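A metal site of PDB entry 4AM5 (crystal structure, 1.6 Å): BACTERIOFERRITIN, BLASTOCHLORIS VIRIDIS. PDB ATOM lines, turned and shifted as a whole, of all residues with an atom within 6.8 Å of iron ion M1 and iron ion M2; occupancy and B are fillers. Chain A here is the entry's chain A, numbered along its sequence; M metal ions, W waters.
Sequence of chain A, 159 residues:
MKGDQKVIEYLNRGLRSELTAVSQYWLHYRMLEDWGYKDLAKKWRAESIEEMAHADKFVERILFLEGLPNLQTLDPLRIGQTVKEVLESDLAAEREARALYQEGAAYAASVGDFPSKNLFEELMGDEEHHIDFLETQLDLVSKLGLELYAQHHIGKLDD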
ATOM      1  N   SER A  17       2.747  26.190 -33.009  1.00  0.00           N
ATOM      2  CA  SER A  17       2.541  25.993 -31.576  1.00  0.00           C
ATOM      3  C   SER A  17       2.565  24.515 -31.174  1.00  0.00           C
ATOM      4  O   SER A  17       3.237  24.165 -30.183  1.00  0.00           O
ATOM      5  CB  SER A  17       1.220  26.650 -31.220  1.00  0.00           C
ATOM      6  OG  SER A  17       1.198  26.690 -29.784  1.00  0.00           O
ATOM      7  N   GLU A  18       1.839  23.693 -31.948  1.00  0.00           N
ATOM      8  CA  GLU A  18       1.816  22.279 -31.592  1.00  0.00           C
ATOM      9  C   GLU A  18       3.142  21.575 -31.818  1.00  0.00           C
ATOM     10  O   GLU A  18       3.515  20.735 -31.028  1.00  0.00           O
ATOM     11  CB  GLU A  18       0.750  21.555 -32.416  1.00  0.00           C
ATOM     12  CG  GLU A  18      -0.663  21.977 -32.084  1.00  0.00           C
ATOM     13  CD  GLU A  18      -1.104  21.599 -30.682  1.00  0.00           C
ATOM     14  OE1 GLU A  18      -0.542  20.687 -30.098  1.00  0.00           O
ATOM     15  OE2 GLU A  18      -2.099  22.144 -30.193  1.00  0.00           O
ATOM     16  N   ALA A  21       4.997  22.273 -28.790  1.00  0.00           N
ATOM     17  CA  ALA A  21       4.550  21.475 -27.644  1.00  0.00           C
ATOM     18  C   ALA A  21       4.996  20.044 -27.754  1.00  0.00           C
ATOM     19  O   ALA A  21       5.338  19.422 -26.745  1.00  0.00           O
ATOM     20  CB  ALA A  21       3.024  21.512 -27.564  1.00  0.00           C
ATOM     21  N   TYR A  25       7.259  18.850 -24.704  1.00  0.00           N
ATOM     22  CA  TYR A  25       6.861  17.694 -23.867  1.00  0.00           C
ATOM     23  C   TYR A  25       7.752  16.483 -24.090  1.00  0.00           C
ATOM     24  O   TYR A  25       8.002  15.744 -23.094  1.00  0.00           O
ATOM     25  CB  TYR A  25       5.379  17.311 -24.172  1.00  0.00           C
ATOM     26  CG  TYR A  25       4.326  18.131 -23.461  1.00  0.00           C
ATOM     27  CD1 TYR A  25       4.286  18.164 -22.059  1.00  0.00           C
ATOM     28  CD2 TYR A  25       3.348  18.803 -24.200  1.00  0.00           C
ATOM     29  CE1 TYR A  25       3.291  18.889 -21.401  1.00  0.00           C
ATOM     30  CE2 TYR A  25       2.356  19.574 -23.550  1.00  0.00           C
ATOM     31  CZ  TYR A  25       2.323  19.604 -22.184  1.00  0.00           C
ATOM     32  OH  TYR A  25       1.266  20.266 -21.558  1.00  0.00           O
ATOM     33  N   GLU A  47       1.297  13.133 -23.020  1.00  0.00           N
ATOM     34  CA  GLU A  47       0.867  14.492 -23.430  1.00  0.00           C
ATOM     35  C   GLU A  47       1.520  14.885 -24.750  1.00  0.00           C
ATOM     36  O   GLU A  47       0.869  15.495 -25.601  1.00  0.00           O
ATOM     37  CB  GLU A  47       1.220  15.557 -22.376  1.00  0.00           C
ATOM     38  CG  GLU A  47       0.507  15.261 -21.075  1.00  0.00           C
ATOM     39  CD  GLU A  47      -1.000  15.604 -21.130  1.00  0.00           C
ATOM     40  OE1 GLU A  47      -1.702  15.473 -22.190  1.00  0.00           O
ATOM     41  OE2 GLU A  47      -1.430  16.134 -20.008  1.00  0.00           O
ATOM     42  N   GLU A  50      -0.457  13.344 -27.455  1.00  0.00           N
ATOM     43  CA  GLU A  50      -1.744  14.105 -27.676  1.00  0.00           C
ATOM     44  C   GLU A  50      -1.399  15.335 -28.567  1.00  0.00           C
ATOM     45  O   GLU A  50      -2.217  15.683 -29.456  1.00  0.00           O
ATOM     46  CB  GLU A  50      -2.343  14.620 -26.347  1.00  0.00           C
ATOM     47  CG  GLU A  50      -2.864  13.472 -25.528  1.00  0.00           C
ATOM     48  CD  GLU A  50      -3.661  13.917 -24.310  1.00  0.00           C
ATOM     49  OE1 GLU A  50      -4.263  15.054 -24.314  1.00  0.00           O
ATOM     50  OE2 GLU A  50      -3.824  13.001 -23.442  1.00  0.00           O
ATOM     51  N   GLU A  51      -0.257  16.019 -28.334  1.00  0.00           N
ATOM     52  CA  GLU A  51      -0.011  17.250 -29.145  1.00  0.00           C
ATOM     53  C   GLU A  51       0.341  16.800 -30.577  1.00  0.00           C
ATOM     54  O   GLU A  51       0.118  17.559 -31.530  1.00  0.00           O
ATOM     55  CB  GLU A  51       1.166  18.072 -28.555  1.00  0.00           C
ATOM     56  CG  GLU A  51       0.980  18.503 -27.087  1.00  0.00           C
ATOM     57  CD  GLU A  51      -0.202  19.258 -26.716  1.00  0.00           C
ATOM     58  OE1 GLU A  51      -1.172  19.281 -27.411  1.00  0.00           O
ATOM     59  OE2 GLU A  51      -0.091  19.909 -25.680  1.00  0.00           O
ATOM     60  N   MET A  52       0.931  15.606 -30.780  1.00  0.00           N
ATOM     61  CA  MET A  52       1.242  15.117 -32.128  1.00  0.00           C
ATOM     62  C   MET A  52      -0.119  15.014 -32.890  1.00  0.00           C
ATOM     63  O   MET A  52      -0.161  15.358 -34.112  1.00  0.00           O
ATOM     64  CB  MET A  52       1.941  13.744 -32.082  1.00  0.00           C
ATOM     65  CG  MET A  52       3.397  13.891 -31.506  1.00  0.00           C
ATOM     66  SD  MET A  52       4.064  12.211 -31.331  1.00  0.00           S
ATOM     67  CE  MET A  52       5.281  12.541 -30.017  1.00  0.00           C
ATOM     68  N   HIS A  54      -2.800  16.767 -32.418  1.00  0.00           N
ATOM     69  CA  HIS A  54      -3.230  18.152 -32.716  1.00  0.00           C
ATOM     70  C   HIS A  54      -2.441  18.706 -33.899  1.00  0.00           C
ATOM     71  O   HIS A  54      -3.038  19.333 -34.797  1.00  0.00           O
ATOM     72  CB  HIS A  54      -2.891  19.065 -31.565  1.00  0.00           C
ATOM     73  CG  HIS A  54      -3.755  18.894 -30.339  1.00  0.00           C
ATOM     74  ND1 HIS A  54      -3.535  19.591 -29.088  1.00  0.00           N
ATOM     75  CD2 HIS A  54      -4.952  18.220 -30.233  1.00  0.00           C
ATOM     76  CE1 HIS A  54      -4.615  19.256 -28.276  1.00  0.00           C
ATOM     77  NE2 HIS A  54      -5.417  18.408 -28.919  1.00  0.00           N
ATOM     78  N   ALA A  55      -1.115  18.500 -33.946  1.00  0.00           N
ATOM     79  CA  ALA A  55      -0.314  18.990 -35.093  1.00  0.00           C
ATOM     80  C   ALA A  55      -0.869  18.381 -36.387  1.00  0.00           C
ATOM     81  O   ALA A  55      -1.011  19.106 -37.397  1.00  0.00           O
ATOM     82  CB  ALA A  55       1.147  18.606 -34.860  1.00  0.00           C
ATOM     83  N   PHE A  58      -3.938  20.040 -37.656  1.00  0.00           N
ATOM     84  CA  PHE A  58      -3.705  21.301 -38.405  1.00  0.00           C
ATOM     85  C   PHE A  58      -3.173  21.058 -39.793  1.00  0.00           C
ATOM     86  O   PHE A  58      -3.601  21.743 -40.740  1.00  0.00           O
ATOM     87  CB  PHE A  58      -2.731  22.210 -37.616  1.00  0.00           C
ATOM     88  CG  PHE A  58      -3.371  22.932 -36.462  1.00  0.00           C
ATOM     89  CD1 PHE A  58      -4.512  23.701 -36.649  1.00  0.00           C
ATOM     90  CD2 PHE A  58      -2.767  22.912 -35.184  1.00  0.00           C
ATOM     91  CE1 PHE A  58      -5.063  24.448 -35.599  1.00  0.00           C
ATOM     92  CE2 PHE A  58      -3.302  23.685 -34.126  1.00  0.00           C
ATOM     93  CZ  PHE A  58      -4.500  24.438 -34.338  1.00  0.00           C
ATOM     94  N   GLU A  94       1.581  26.319 -22.749  1.00  0.00           N
ATOM     95  CA  GLU A  94       0.185  25.940 -23.003  1.00  0.00           C
ATOM     96  C   GLU A  94      -0.789  27.138 -22.859  1.00  0.00           C
ATOM     97  O   GLU A  94      -1.761  27.184 -23.601  1.00  0.00           O
ATOM     98  CB  GLU A  94      -0.153  24.794 -22.046  1.00  0.00           C
ATOM     99  CG  GLU A  94       0.736  23.564 -22.317  1.00  0.00           C
ATOM    100  CD  GLU A  94       0.230  22.704 -23.473  1.00  0.00           C
ATOM    101  OE1 GLU A  94       0.438  23.096 -24.668  1.00  0.00           O
ATOM    102  OE2 GLU A  94      -0.405  21.633 -23.133  1.00  0.00           O
ATOM    103  N   ALA A  97      -0.633  28.718 -26.201  1.00  0.00           N
ATOM    104  CA  ALA A  97      -1.446  27.988 -27.184  1.00  0.00           C
ATOM    105  C   ALA A  97      -2.950  28.238 -27.066  1.00  0.00           C
ATOM    106  O   ALA A  97      -3.633  28.432 -28.069  1.00  0.00           O
ATOM    107  CB  ALA A  97      -1.126  26.474 -27.068  1.00  0.00           C
ATOM    108  N   TYR A 101      -5.483  29.795 -29.855  1.00  0.00           N
ATOM    109  CA  TYR A 101      -6.687  29.159 -30.388  1.00  0.00           C
ATOM    110  C   TYR A 101      -7.981  29.915 -30.146  1.00  0.00           C
ATOM    111  O   TYR A 101      -8.917  29.834 -30.990  1.00  0.00           O
ATOM    112  CB  TYR A 101      -6.792  27.678 -29.808  1.00  0.00           C
ATOM    113  CG  TYR A 101      -5.555  26.855 -30.155  1.00  0.00           C
ATOM    114  CD1 TYR A 101      -4.689  27.221 -31.142  1.00  0.00           C
ATOM    115  CD2 TYR A 101      -5.255  25.711 -29.389  1.00  0.00           C
ATOM    116  CE1 TYR A 101      -3.507  26.530 -31.378  1.00  0.00           C
ATOM    117  CE2 TYR A 101      -4.110  24.939 -29.636  1.00  0.00           C
ATOM    118  CZ  TYR A 101      -3.223  25.360 -30.620  1.00  0.00           C
ATOM    119  OH  TYR A 101      -2.106  24.594 -30.835  1.00  0.00           O
ATOM    120  N   LEU A 123      -9.455  22.290 -29.870  1.00  0.00           N
ATOM    121  CA  LEU A 123      -8.087  22.308 -29.314  1.00  0.00           C
ATOM    122  C   LEU A 123      -8.028  23.272 -28.127  1.00  0.00           C
ATOM    123  O   LEU A 123      -7.247  22.994 -27.171  1.00  0.00           O
ATOM    124  CB  LEU A 123      -7.075  22.679 -30.424  1.00  0.00           C
ATOM    125  CG  LEU A 123      -6.550  21.367 -31.113  1.00  0.00           C
ATOM    126  CD1 LEU A 123      -7.582  20.384 -31.578  1.00  0.00           C
ATOM    127  CD2 LEU A 123      -5.702  21.788 -32.336  1.00  0.00           C
ATOM    128  N   ASP A 126      -8.978  21.299 -25.273  1.00  0.00           N
ATOM    129  CA  ASP A 126      -8.001  20.321 -24.850  1.00  0.00           C
ATOM    130  C   ASP A 126      -6.811  20.995 -24.153  1.00  0.00           C
ATOM    131  O   ASP A 126      -6.310  20.434 -23.207  1.00  0.00           O
ATOM    132  CB  ASP A 126      -7.446  19.664 -26.109  1.00  0.00           C
ATOM    133  CG  ASP A 126      -8.417  18.751 -26.804  1.00  0.00           C
ATOM    134  OD1 ASP A 126      -9.437  18.281 -26.176  1.00  0.00           O
ATOM    135  OD2 ASP A 126      -8.123  18.333 -27.993  1.00  0.00           O
ATOM    136  N   GLU A 127      -6.422  22.195 -24.641  1.00  0.00           N
ATOM    137  CA  GLU A 127      -5.315  22.846 -23.958  1.00  0.00           C
ATOM    138  C   GLU A 127      -5.762  23.338 -22.575  1.00  0.00           C
ATOM    139  O   GLU A 127      -4.873  23.367 -21.644  1.00  0.00           O
ATOM    140  CB  GLU A 127      -4.732  24.055 -24.722  1.00  0.00           C
ATOM    141  CG  GLU A 127      -4.280  23.695 -26.132  1.00  0.00           C
ATOM    142  CD  GLU A 127      -3.425  22.440 -26.163  1.00  0.00           C
ATOM    143  OE1 GLU A 127      -2.647  22.215 -25.200  1.00  0.00           O
ATOM    144  OE2 GLU A 127      -3.417  21.986 -27.312  1.00  0.00           O
ATOM    145  N   GLU A 128      -7.042  23.701 -22.349  1.00  0.00           N
ATOM    146  CA  GLU A 128      -7.393  24.038 -20.972  1.00  0.00           C
ATOM    147  C   GLU A 128      -7.335  22.801 -20.055  1.00  0.00           C
ATOM    148  O   GLU A 128      -6.985  22.954 -18.901  1.00  0.00           O
ATOM    149  CB  GLU A 128      -8.808  24.633 -20.969  1.00  0.00           C
ATOM    150  CG  GLU A 128      -8.735  26.126 -21.431  1.00  0.00           C
ATOM    151  CD  GLU A 128     -10.003  26.883 -21.337  1.00  0.00           C
ATOM    152  OE1 GLU A 128     -10.967  26.377 -20.763  1.00  0.00           O
ATOM    153  OE2 GLU A 128     -10.017  28.080 -21.749  1.00  0.00           O
ATOM    154  N   HIS A 130      -5.013  20.442 -20.441  1.00  0.00           N
ATOM    155  CA  HIS A 130      -3.568  20.379 -20.115  1.00  0.00           C
ATOM    156  C   HIS A 130      -3.146  21.410 -19.109  1.00  0.00           C
ATOM    157  O   HIS A 130      -2.327  21.126 -18.230  1.00  0.00           O
ATOM    158  CB  HIS A 130      -2.737  20.579 -21.404  1.00  0.00           C
ATOM    159  CG  HIS A 130      -2.927  19.467 -22.404  1.00  0.00           C
ATOM    160  ND1 HIS A 130      -2.517  19.545 -23.742  1.00  0.00           N
ATOM    161  CD2 HIS A 130      -3.616  18.248 -22.266  1.00  0.00           C
ATOM    162  CE1 HIS A 130      -2.891  18.397 -24.384  1.00  0.00           C
ATOM    163  NE2 HIS A 130      -3.562  17.603 -23.516  1.00  0.00           N
ATOM    164  N   ILE A 131      -3.662  22.647 -19.221  1.00  0.00           N
ATOM    165  CA  ILE A 131      -3.422  23.707 -18.249  1.00  0.00           C
ATOM    166  C   ILE A 131      -3.895  23.252 -16.832  1.00  0.00           C
ATOM    167  O   ILE A 131      -3.169  23.475 -15.854  1.00  0.00           O
ATOM    168  CB  ILE A 131      -4.131  25.030 -18.713  1.00  0.00           C
ATOM    169  CG1 ILE A 131      -3.281  25.584 -19.855  1.00  0.00           C
ATOM    170  CG2 ILE A 131      -4.219  26.066 -17.573  1.00  0.00           C
ATOM    171  CD1 ILE A 131      -4.096  26.623 -20.651  1.00  0.00           C
ATOM    172  N   LEU A 134      -1.366  20.843 -15.363  1.00  0.00           N
ATOM    173  CA  LEU A 134      -0.147  21.479 -14.969  1.00  0.00           C
ATOM    174  C   LEU A 134      -0.309  22.418 -13.753  1.00  0.00           C
ATOM    175  O   LEU A 134       0.512  22.351 -12.826  1.00  0.00           O
ATOM    176  CB  LEU A 134       0.439  22.335 -16.101  1.00  0.00           C
ATOM    177  CG  LEU A 134       0.870  21.436 -17.277  1.00  0.00           C
ATOM    178  CD1 LEU A 134       1.074  22.276 -18.623  1.00  0.00           C
ATOM    179  CD2 LEU A 134       2.159  20.572 -16.997  1.00  0.00           C
HETATM  180 FE    FE M   1      -1.448  20.951 -24.682  1.00  0.00          FE
HETATM  181 FE    FE M   2      -2.039  20.857 -28.452  1.00  0.00          FE
HETATM  182  O   HOH W   1      -0.367  22.294 -27.543  1.00  0.00           O
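Iron ion M1 is bound by the side-chain carboxylate (OE1) of Glu 127 (1.8 Å).
Iron ion M1 is bound by the side-chain carboxylate (OE2) of Glu 51, 2.0 Å away.
OE2 of Glu 94 binds iron ion M1, at 2.0 Å.
Iron ion M1 is bound by ND1 of His 130, 2.0 Å away.
Iron ion M1 has four donor atoms within binding distance.
ND1 of His 54 binds iron ion M2.
Iron ion M2 is bound by OE1 of Glu 51 (2.1 Å).
Iron ion M2 is bound by OE2 of Glu 127 (2.1 Å).
Iron ion M2 is bound by OE2 of Glu 18, at 2.2 Å.
Iron ion M2 is bound by the side-chain carboxylate (OE1) of Glu 18 (2.2 Å).
Water W1 binds iron ion M2.
Iron ion M2 has six donor atoms within binding distance.
The nearest printed residue that does not touch iron ion M2 is Tyr 101 (4.4 Å).
Of the 21 residues printed, 4 come within 4 Å of iron ion M1.
The nearest printed residue that does not touch iron ion M1 is Tyr 25 (4.2 Å).
The side-chain carboxylate (OD2) of Asp 126 lies within hydrogen-bond range of a ring nitrogen (NE2) of His 54, at 2.9 Å.
OE1 of Glu 50 is in hydrogen-bond range of NE2 of His 130, at 2.8 Å.
The side-chain carboxylate (OE2) of Glu 18 sits close to the side-chain hydroxyl (OH) of Tyr 101, 2.5 Å away.
The side-chain carboxylate (OE2) of Glu 94 sits close to the side-chain hydroxyl (OH) of Tyr 25 (2.7 Å).
A ring nitrogen (NE2) of His 130 sits at hydrogen-bond distance from the side-chain carboxylate (OE1) of Glu 47 (3.1 Å).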
